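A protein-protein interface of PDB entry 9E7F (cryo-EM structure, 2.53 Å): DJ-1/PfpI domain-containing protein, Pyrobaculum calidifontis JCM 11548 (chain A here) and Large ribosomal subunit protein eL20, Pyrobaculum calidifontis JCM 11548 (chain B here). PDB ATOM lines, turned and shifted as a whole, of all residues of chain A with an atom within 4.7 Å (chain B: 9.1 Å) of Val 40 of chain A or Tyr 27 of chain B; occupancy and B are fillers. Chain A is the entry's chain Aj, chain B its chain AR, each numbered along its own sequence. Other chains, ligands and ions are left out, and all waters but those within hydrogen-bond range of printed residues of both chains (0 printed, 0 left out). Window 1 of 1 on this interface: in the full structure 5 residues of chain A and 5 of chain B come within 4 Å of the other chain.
O of Arg 38 of chain A touches CD1 of Tyr 27 of chain B (3.4 Å).
Val 53 of chain B touches Arg 38 of chain A.
Tyr 27 of chain B touches Val 40 of chain A (CG to O, 3.4 Å).
Tyr 27 of chain B touches Asn 41 of chain A.
The guanidinium group (NH2) of Arg 25 of chain B sits at hydrogen-bond distance from the backbone carbonyl oxygen (O) of Asn 41 of chain A.
Of the 17 printed residues of chain B, 3 touch a printed residue of chain A.
Hydrophobic or aromatic side chains of chain B within 4 Å of the printed part of chain A: Tyr 27 and Val 53.
Along chain A the printed residues that touch a printed residue of chain B span positions 38 to 41.
Among the printed residues, no Asp or Glu carboxylate lies within 4 Å of a Lys or Arg side-chain nitrogen of the other chain.
Of chain B, only Tyr 27 (3.4 Å) comes within 4 Å of Val 40 of chain A.
Tyr 27 of chain B touches just these residues of chain A: Arg 38 (3.4 Å), Val 40 (3.4 Å) and Asn 41 (3.4 Å).
No residue of chain B comes within 4 Å of Asp 39 of chain A.
Of the printed residues of chain A, Arg 25 of chain B touches Asn 41 (3.1 Å).
Printed residues of chain B within 4 Å of Asn 41 of chain A: Arg 25 (3.1 Å) and Tyr 27 (3.4 Å).
Of the printed residues of chain B, Arg 38 of chain A touches Tyr 27 (3.4 Å) and Val 53 (3.8 Å).
Printed residues of chain A within 4 Å of Val 53 of chain B: Arg 38.
The nearest printed residue of chain B that does not touch Asn 41 of chain A is Asp 28 of chain B (7.1 Å).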
ATOM      1  N   VAL A   8      25.135 -22.973  -3.055  1.00  0.00           N
ATOM      2  CA  VAL A   8      24.265 -22.490  -4.123  1.00  0.00           C
ATOM      3  C   VAL A   8      25.178 -22.119  -5.285  1.00  0.00           C
ATOM      4  O   VAL A   8      25.614 -20.977  -5.420  1.00  0.00           O
ATOM      5  CB  VAL A   8      23.404 -21.315  -3.668  1.00  0.00           C
ATOM      6  CG1 VAL A   8      22.383 -20.962  -4.726  1.00  0.00           C
ATOM      7  CG2 VAL A   8      22.711 -21.643  -2.363  1.00  0.00           C
ATOM      8  N   ILE A   9      25.477 -23.099  -6.138  1.00  0.00           N
ATOM      9  CA  ILE A   9      26.306 -22.824  -7.306  1.00  0.00           C
ATOM     10  C   ILE A   9      25.517 -22.040  -8.345  1.00  0.00           C
ATOM     11  O   ILE A   9      26.064 -21.178  -9.041  1.00  0.00           O
ATOM     12  CB  ILE A   9      26.870 -24.126  -7.902  1.00  0.00           C
ATOM     13  CG1 ILE A   9      27.939 -24.733  -6.998  1.00  0.00           C
ATOM     14  CG2 ILE A   9      27.469 -23.860  -9.266  1.00  0.00           C
ATOM     15  CD1 ILE A   9      27.406 -25.574  -5.882  1.00  0.00           C
ATOM     16  N   THR A  11      21.404 -20.384  -9.657  1.00  0.00           N
ATOM     17  CA  THR A  11      20.009 -20.033  -9.420  1.00  0.00           C
ATOM     18  C   THR A  11      19.202 -19.996 -10.713  1.00  0.00           C
ATOM     19  O   THR A  11      18.116 -19.408 -10.739  1.00  0.00           O
ATOM     20  CB  THR A  11      19.892 -18.695  -8.688  1.00  0.00           C
ATOM     21  OG1 THR A  11      20.867 -17.777  -9.192  1.00  0.00           O
ATOM     22  CG2 THR A  11      20.087 -18.886  -7.198  1.00  0.00           C
ATOM     23  N   VAL A  35      28.450 -19.524  -1.129  1.00  0.00           N
ATOM     24  CA  VAL A  35      28.438 -19.068  -2.512  1.00  0.00           C
ATOM     25  C   VAL A  35      29.876 -18.931  -2.990  1.00  0.00           C
ATOM     26  O   VAL A  35      30.753 -18.469  -2.256  1.00  0.00           O
ATOM     27  CB  VAL A  35      27.668 -17.736  -2.658  1.00  0.00           C
ATOM     28  CG1 VAL A  35      27.913 -17.110  -4.011  1.00  0.00           C
ATOM     29  CG2 VAL A  35      26.193 -17.961  -2.447  1.00  0.00           C
ATOM     30  N   SER A  37      30.516 -17.711  -6.418  1.00  0.00           N
ATOM     31  CA  SER A  37      30.523 -16.914  -7.636  1.00  0.00           C
ATOM     32  C   SER A  37      29.686 -15.665  -7.415  1.00  0.00           C
ATOM     33  O   SER A  37      28.863 -15.601  -6.501  1.00  0.00           O
ATOM     34  CB  SER A  37      30.004 -17.710  -8.837  1.00  0.00           C
ATOM     35  OG  SER A  37      28.595 -17.811  -8.812  1.00  0.00           O
ATOM     36  N   ARG A  38      29.909 -14.667  -8.266  1.00  0.00           N
ATOM     37  CA  ARG A  38      29.274 -13.364  -8.119  1.00  0.00           C
ATOM     38  C   ARG A  38      27.950 -13.244  -8.863  1.00  0.00           C
ATOM     39  O   ARG A  38      27.322 -12.185  -8.802  1.00  0.00           O
ATOM     40  CB  ARG A  38      30.218 -12.259  -8.594  1.00  0.00           C
ATOM     41  CG  ARG A  38      31.640 -12.386  -8.091  1.00  0.00           C
ATOM     42  CD  ARG A  38      32.563 -11.510  -8.905  1.00  0.00           C
ATOM     43  NE  ARG A  38      32.116 -11.426 -10.290  1.00  0.00           N
ATOM     44  CZ  ARG A  38      32.926 -11.405 -11.338  1.00  0.00           C
ATOM     45  NH1 ARG A  38      34.241 -11.440 -11.196  1.00  0.00           N
ATOM     46  NH2 ARG A  38      32.403 -11.342 -12.559  1.00  0.00           N
ATOM     47  N   ASP A  39      27.508 -14.283  -9.560  1.00  0.00           N
ATOM     48  CA  ASP A  39      26.242 -14.224 -10.274  1.00  0.00           C
ATOM     49  C   ASP A  39      25.071 -14.718  -9.443  1.00  0.00           C
ATOM     50  O   ASP A  39      23.948 -14.764  -9.953  1.00  0.00           O
ATOM     51  CB  ASP A  39      26.321 -15.038 -11.564  1.00  0.00           C
ATOM     52  CG  ASP A  39      27.043 -16.347 -11.373  1.00  0.00           C
ATOM     53  OD1 ASP A  39      28.144 -16.330 -10.789  1.00  0.00           O
ATOM     54  OD2 ASP A  39      26.511 -17.393 -11.796  1.00  0.00           O
ATOM     55  N   VAL A  40      25.295 -15.090  -8.191  1.00  0.00           N
ATOM     56  CA  VAL A  40      24.236 -15.621  -7.342  1.00  0.00           C
ATOM     57  C   VAL A  40      23.645 -14.485  -6.522  1.00  0.00           C
ATOM     58  O   VAL A  40      24.374 -13.704  -5.903  1.00  0.00           O
ATOM     59  CB  VAL A  40      24.766 -16.746  -6.442  1.00  0.00           C
ATOM     60  CG1 VAL A  40      23.652 -17.297  -5.583  1.00  0.00           C
ATOM     61  CG2 VAL A  40      25.375 -17.842  -7.286  1.00  0.00           C
ATOM     62  N   ASN A  41      22.317 -14.395  -6.518  1.00  0.00           N
ATOM     63  CA  ASN A  41      21.602 -13.291  -5.898  1.00  0.00           C
ATOM     64  C   ASN A  41      21.147 -13.570  -4.473  1.00  0.00           C
ATOM     65  O   ASN A  41      20.705 -12.639  -3.793  1.00  0.00           O
ATOM     66  CB  ASN A  41      20.382 -12.925  -6.746  1.00  0.00           C
ATOM     67  CG  ASN A  41      19.336 -14.009  -6.751  1.00  0.00           C
ATOM     68  OD1 ASN A  41      19.589 -15.124  -7.202  1.00  0.00           O
ATOM     69  ND2 ASN A  41      18.153 -13.693  -6.250  1.00  0.00           N
ATOM     70  N   VAL A  42      21.240 -14.805  -4.005  1.00  0.00           N
ATOM     71  CA  VAL A  42      20.694 -15.153  -2.700  1.00  0.00           C
ATOM     72  C   VAL A  42      21.614 -14.636  -1.608  1.00  0.00           C
ATOM     73  O   VAL A  42      22.813 -14.428  -1.817  1.00  0.00           O
ATOM     74  CB  VAL A  42      20.488 -16.674  -2.576  1.00  0.00           C
ATOM     75  CG1 VAL A  42      19.980 -17.247  -3.880  1.00  0.00           C
ATOM     76  CG2 VAL A  42      21.775 -17.343  -2.149  1.00  0.00           C
ATOM     77  N   TYR B   5      33.906  -1.952  -3.510  1.00  0.00           N
ATOM     78  CA  TYR B   5      34.370  -2.977  -4.435  1.00  0.00           C
ATOM     79  C   TYR B   5      34.933  -2.304  -5.675  1.00  0.00           C
ATOM     80  O   TYR B   5      34.229  -1.540  -6.340  1.00  0.00           O
ATOM     81  CB  TYR B   5      33.232  -3.913  -4.820  1.00  0.00           C
ATOM     82  CG  TYR B   5      32.754  -4.807  -3.711  1.00  0.00           C
ATOM     83  CD1 TYR B   5      31.532  -4.578  -3.094  1.00  0.00           C
ATOM     84  CD2 TYR B   5      33.501  -5.897  -3.300  1.00  0.00           C
ATOM     85  CE1 TYR B   5      31.080  -5.397  -2.087  1.00  0.00           C
ATOM     86  CE2 TYR B   5      33.054  -6.722  -2.299  1.00  0.00           C
ATOM     87  CZ  TYR B   5      31.848  -6.466  -1.693  1.00  0.00           C
ATOM     88  OH  TYR B   5      31.402  -7.287  -0.688  1.00  0.00           O
ATOM     89  N   VAL B   7      35.665  -2.483  -9.168  1.00  0.00           N
ATOM     90  CA  VAL B   7      35.327  -3.230 -10.373  1.00  0.00           C
ATOM     91  C   VAL B   7      36.220  -2.769 -11.515  1.00  0.00           C
ATOM     92  O   VAL B   7      36.332  -1.569 -11.786  1.00  0.00           O
ATOM     93  CB  VAL B   7      33.846  -3.049 -10.732  1.00  0.00           C
ATOM     94  CG1 VAL B   7      33.493  -3.894 -11.936  1.00  0.00           C
ATOM     95  CG2 VAL B   7      32.977  -3.417  -9.555  1.00  0.00           C
ATOM     96  N   VAL B  21      32.372   0.788  -6.176  1.00  0.00           N
ATOM     97  CA  VAL B  21      30.974   0.733  -5.775  1.00  0.00           C
ATOM     98  C   VAL B  21      30.900   0.268  -4.330  1.00  0.00           C
ATOM     99  O   VAL B  21      31.623  -0.642  -3.913  1.00  0.00           O
ATOM    100  CB  VAL B  21      30.152  -0.194  -6.701  1.00  0.00           C
ATOM    101  CG1 VAL B  21      28.884  -0.644  -6.020  1.00  0.00           C
ATOM    102  CG2 VAL B  21      29.828   0.510  -7.997  1.00  0.00           C
ATOM    103  N   GLY B  23      28.740  -1.679  -1.983  1.00  0.00           N
ATOM    104  CA  GLY B  23      27.653  -2.634  -2.000  1.00  0.00           C
ATOM    105  C   GLY B  23      27.820  -3.666  -0.904  1.00  0.00           C
ATOM    106  O   GLY B  23      28.923  -3.923  -0.421  1.00  0.00           O
ATOM    107  N   GLU B  24      26.690  -4.258  -0.518  1.00  0.00           N
ATOM    108  CA  GLU B  24      26.695  -5.235   0.566  1.00  0.00           C
ATOM    109  C   GLU B  24      27.457  -6.497   0.183  1.00  0.00           C
ATOM    110  O   GLU B  24      28.233  -7.025   0.986  1.00  0.00           O
ATOM    111  CB  GLU B  24      25.261  -5.571   0.963  1.00  0.00           C
ATOM    112  CG  GLU B  24      25.113  -6.132   2.358  1.00  0.00           C
ATOM    113  CD  GLU B  24      23.776  -6.817   2.557  1.00  0.00           C
ATOM    114  OE1 GLU B  24      22.754  -6.228   2.161  1.00  0.00           O
ATOM    115  OE2 GLU B  24      23.745  -7.940   3.102  1.00  0.00           O
ATOM    116  N   ARG B  25      27.252  -6.994  -1.027  1.00  0.00           N
ATOM    117  CA  ARG B  25      27.970  -8.146  -1.545  1.00  0.00           C
ATOM    118  C   ARG B  25      28.381  -7.844  -2.975  1.00  0.00           C
ATOM    119  O   ARG B  25      27.888  -6.881  -3.573  1.00  0.00           O
ATOM    120  CB  ARG B  25      27.120  -9.423  -1.487  1.00  0.00           C
ATOM    121  CG  ARG B  25      25.754  -9.295  -2.108  1.00  0.00           C
ATOM    122  CD  ARG B  25      25.042 -10.630  -2.100  1.00  0.00           C
ATOM    123  NE  ARG B  25      23.674 -10.532  -2.592  1.00  0.00           N
ATOM    124  CZ  ARG B  25      22.688  -9.932  -1.944  1.00  0.00           C
ATOM    125  NH1 ARG B  25      22.882  -9.356  -0.770  1.00  0.00           N
ATOM    126  NH2 ARG B  25      21.474  -9.911  -2.486  1.00  0.00           N
ATOM    127  N   PRO B  26      29.312  -8.625  -3.538  1.00  0.00           N
ATOM    128  CA  PRO B  26      29.762  -8.354  -4.917  1.00  0.00           C
ATOM    129  C   PRO B  26      28.658  -8.436  -5.958  1.00  0.00           C
ATOM    130  O   PRO B  26      28.718  -7.726  -6.968  1.00  0.00           O
ATOM    131  CB  PRO B  26      30.832  -9.427  -5.148  1.00  0.00           C
ATOM    132  CG  PRO B  26      31.260  -9.844  -3.808  1.00  0.00           C
ATOM    133  CD  PRO B  26      30.077  -9.715  -2.916  1.00  0.00           C
ATOM    134  N   TYR B  27      27.653  -9.289  -5.748  1.00  0.00           N
ATOM    135  CA  TYR B  27      26.506  -9.310  -6.649  1.00  0.00           C
ATOM    136  C   TYR B  27      25.754  -7.987  -6.607  1.00  0.00           C
ATOM    137  O   TYR B  27      25.266  -7.510  -7.636  1.00  0.00           O
ATOM    138  CB  TYR B  27      25.574 -10.466  -6.290  1.00  0.00           C
ATOM    139  CG  TYR B  27      24.270 -10.455  -7.056  1.00  0.00           C
ATOM    140  CD1 TYR B  27      24.211 -10.911  -8.361  1.00  0.00           C
ATOM    141  CD2 TYR B  27      23.101  -9.990  -6.473  1.00  0.00           C
ATOM    142  CE1 TYR B  27      23.033 -10.900  -9.062  1.00  0.00           C
ATOM    143  CE2 TYR B  27      21.919  -9.969  -7.169  1.00  0.00           C
ATOM    144  CZ  TYR B  27      21.889 -10.428  -8.462  1.00  0.00           C
ATOM    145  OH  TYR B  27      20.706 -10.416  -9.157  1.00  0.00           O
ATOM    146  N   ASP B  28      25.620  -7.402  -5.416  1.00  0.00           N
ATOM    147  CA  ASP B  28      24.958  -6.109  -5.286  1.00  0.00           C
ATOM    148  C   ASP B  28      25.721  -5.020  -6.026  1.00  0.00           C
ATOM    149  O   ASP B  28      25.117  -4.151  -6.664  1.00  0.00           O
ATOM    150  CB  ASP B  28      24.812  -5.751  -3.808  1.00  0.00           C
ATOM    151  CG  ASP B  28      23.907  -4.565  -3.584  1.00  0.00           C
ATOM    152  OD1 ASP B  28      22.800  -4.542  -4.161  1.00  0.00           O
ATOM    153  OD2 ASP B  28      24.302  -3.648  -2.833  1.00  0.00           O
ATOM    154  N   ALA B  29      27.052  -5.044  -5.944  1.00  0.00           N
ATOM    155  CA  ALA B  29      27.858  -4.068  -6.664  1.00  0.00           C
ATOM    156  C   ALA B  29      27.762  -4.270  -8.170  1.00  0.00           C
ATOM    157  O   ALA B  29      27.726  -3.297  -8.929  1.00  0.00           O
ATOM    158  CB  ALA B  29      29.312  -4.153  -6.209  1.00  0.00           C
ATOM    159  N   LEU B  30      27.725  -5.527  -8.618  1.00  0.00           N
ATOM    160  CA  LEU B  30      27.682  -5.813 -10.049  1.00  0.00           C
ATOM    161  C   LEU B  30      26.392  -5.319 -10.687  1.00  0.00           C
ATOM    162  O   LEU B  30      26.391  -4.922 -11.855  1.00  0.00           O
ATOM    163  CB  LEU B  30      27.846  -7.312 -10.283  1.00  0.00           C
ATOM    164  CG  LEU B  30      29.065  -7.779 -11.074  1.00  0.00           C
ATOM    165  CD1 LEU B  30      28.871  -9.214 -11.520  1.00  0.00           C
ATOM    166  CD2 LEU B  30      29.308  -6.879 -12.268  1.00  0.00           C
ATOM    167  N   GLU B  31      25.284  -5.344  -9.948  1.00  0.00           N
ATOM    168  CA  GLU B  31      24.051  -4.765 -10.462  1.00  0.00           C
ATOM    169  C   GLU B  31      24.162  -3.253 -10.593  1.00  0.00           C
ATOM    170  O   GLU B  31      23.507  -2.657 -11.453  1.00  0.00           O
ATOM    171  CB  GLU B  31      22.879  -5.136  -9.557  1.00  0.00           C
ATOM    172  CG  GLU B  31      22.254  -6.490  -9.859  1.00  0.00           C
ATOM    173  CD  GLU B  31      21.609  -6.553 -11.228  1.00  0.00           C
ATOM    174  OE1 GLU B  31      21.911  -7.499 -11.983  1.00  0.00           O
ATOM    175  OE2 GLU B  31      20.800  -5.659 -11.552  1.00  0.00           O
ATOM    176  N   LYS B  32      24.968  -2.618  -9.744  1.00  0.00           N
ATOM    177  CA  LYS B  32      25.171  -1.178  -9.855  1.00  0.00           C
ATOM    178  C   LYS B  32      25.991  -0.823 -11.090  1.00  0.00           C
ATOM    179  O   LYS B  32      25.766   0.222 -11.708  1.00  0.00           O
ATOM    180  CB  LYS B  32      25.844  -0.644  -8.593  1.00  0.00           C
ATOM    181  CG  LYS B  32      25.744   0.859  -8.431  1.00  0.00           C
ATOM    182  CD  LYS B  32      26.067   1.300  -7.011  1.00  0.00           C
ATOM    183  CE  LYS B  32      25.636   0.270  -5.985  1.00  0.00           C
ATOM    184  NZ  LYS B  32      25.247   0.905  -4.698  1.00  0.00           N
ATOM    185  N   VAL B  33      26.960  -1.660 -11.456  1.00  0.00           N
ATOM    186  CA  VAL B  33      27.790  -1.350 -12.614  1.00  0.00           C
ATOM    187  C   VAL B  33      27.007  -1.518 -13.910  1.00  0.00           C
ATOM    188  O   VAL B  33      27.158  -0.725 -14.845  1.00  0.00           O
ATOM    189  CB  VAL B  33      29.067  -2.206 -12.607  1.00  0.00           C
ATOM    190  CG1 VAL B  33      29.827  -2.018 -13.902  1.00  0.00           C
ATOM    191  CG2 VAL B  33      29.942  -1.832 -11.429  1.00  0.00           C
ATOM    192  N   TYR B  34      26.174  -2.559 -13.999  1.00  0.00           N
ATOM    193  CA  TYR B  34      25.451  -2.835 -15.238  1.00  0.00           C
ATOM    194  C   TYR B  34      24.431  -1.748 -15.543  1.00  0.00           C
ATOM    195  O   TYR B  34      24.333  -1.270 -16.678  1.00  0.00           O
ATOM    196  CB  TYR B  34      24.760  -4.192 -15.153  1.00  0.00           C
ATOM    197  CG  TYR B  34      25.694  -5.362 -15.279  1.00  0.00           C
ATOM    198  CD1 TYR B  34      26.689  -5.376 -16.241  1.00  0.00           C
ATOM    199  CD2 TYR B  34      25.584  -6.455 -14.435  1.00  0.00           C
ATOM    200  CE1 TYR B  34      27.547  -6.443 -16.360  1.00  0.00           C
ATOM    201  CE2 TYR B  34      26.436  -7.525 -14.546  1.00  0.00           C
ATOM    202  CZ  TYR B  34      27.417  -7.514 -15.509  1.00  0.00           C
ATOM    203  OH  TYR B  34      28.274  -8.579 -15.625  1.00  0.00           O
ATOM    204  N   ARG B  45      24.252  -5.594 -21.363  1.00  0.00           N
ATOM    205  CA  ARG B  45      25.076  -6.365 -20.440  1.00  0.00           C
ATOM    206  C   ARG B  45      25.978  -7.359 -21.156  1.00  0.00           C
ATOM    207  O   ARG B  45      26.955  -7.824 -20.564  1.00  0.00           O
ATOM    208  CB  ARG B  45      24.190  -7.087 -19.431  1.00  0.00           C
ATOM    209  CG  ARG B  45      23.561  -6.143 -18.445  1.00  0.00           C
ATOM    210  CD  ARG B  45      22.494  -6.798 -17.613  1.00  0.00           C
ATOM    211  NE  ARG B  45      21.821  -5.805 -16.791  1.00  0.00           N
ATOM    212  CZ  ARG B  45      21.608  -5.931 -15.491  1.00  0.00           C
ATOM    213  NH1 ARG B  45      21.979  -7.014 -14.834  1.00  0.00           N
ATOM    214  NH2 ARG B  45      21.009  -4.942 -14.835  1.00  0.00           N
ATOM    215  N   VAL B  53      36.911  -8.145  -9.547  1.00  0.00           N
ATOM    216  CA  VAL B  53      36.218  -7.514  -8.432  1.00  0.00           C
ATOM    217  C   VAL B  53      37.020  -7.786  -7.171  1.00  0.00           C
ATOM    218  O   VAL B  53      37.260  -8.948  -6.826  1.00  0.00           O
ATOM    219  CB  VAL B  53      34.778  -8.030  -8.273  1.00  0.00           C
ATOM    220  CG1 VAL B  53      34.051  -7.225  -7.214  1.00  0.00           C
ATOM    221  CG2 VAL B  53      34.043  -7.971  -9.595  1.00  0.00           C
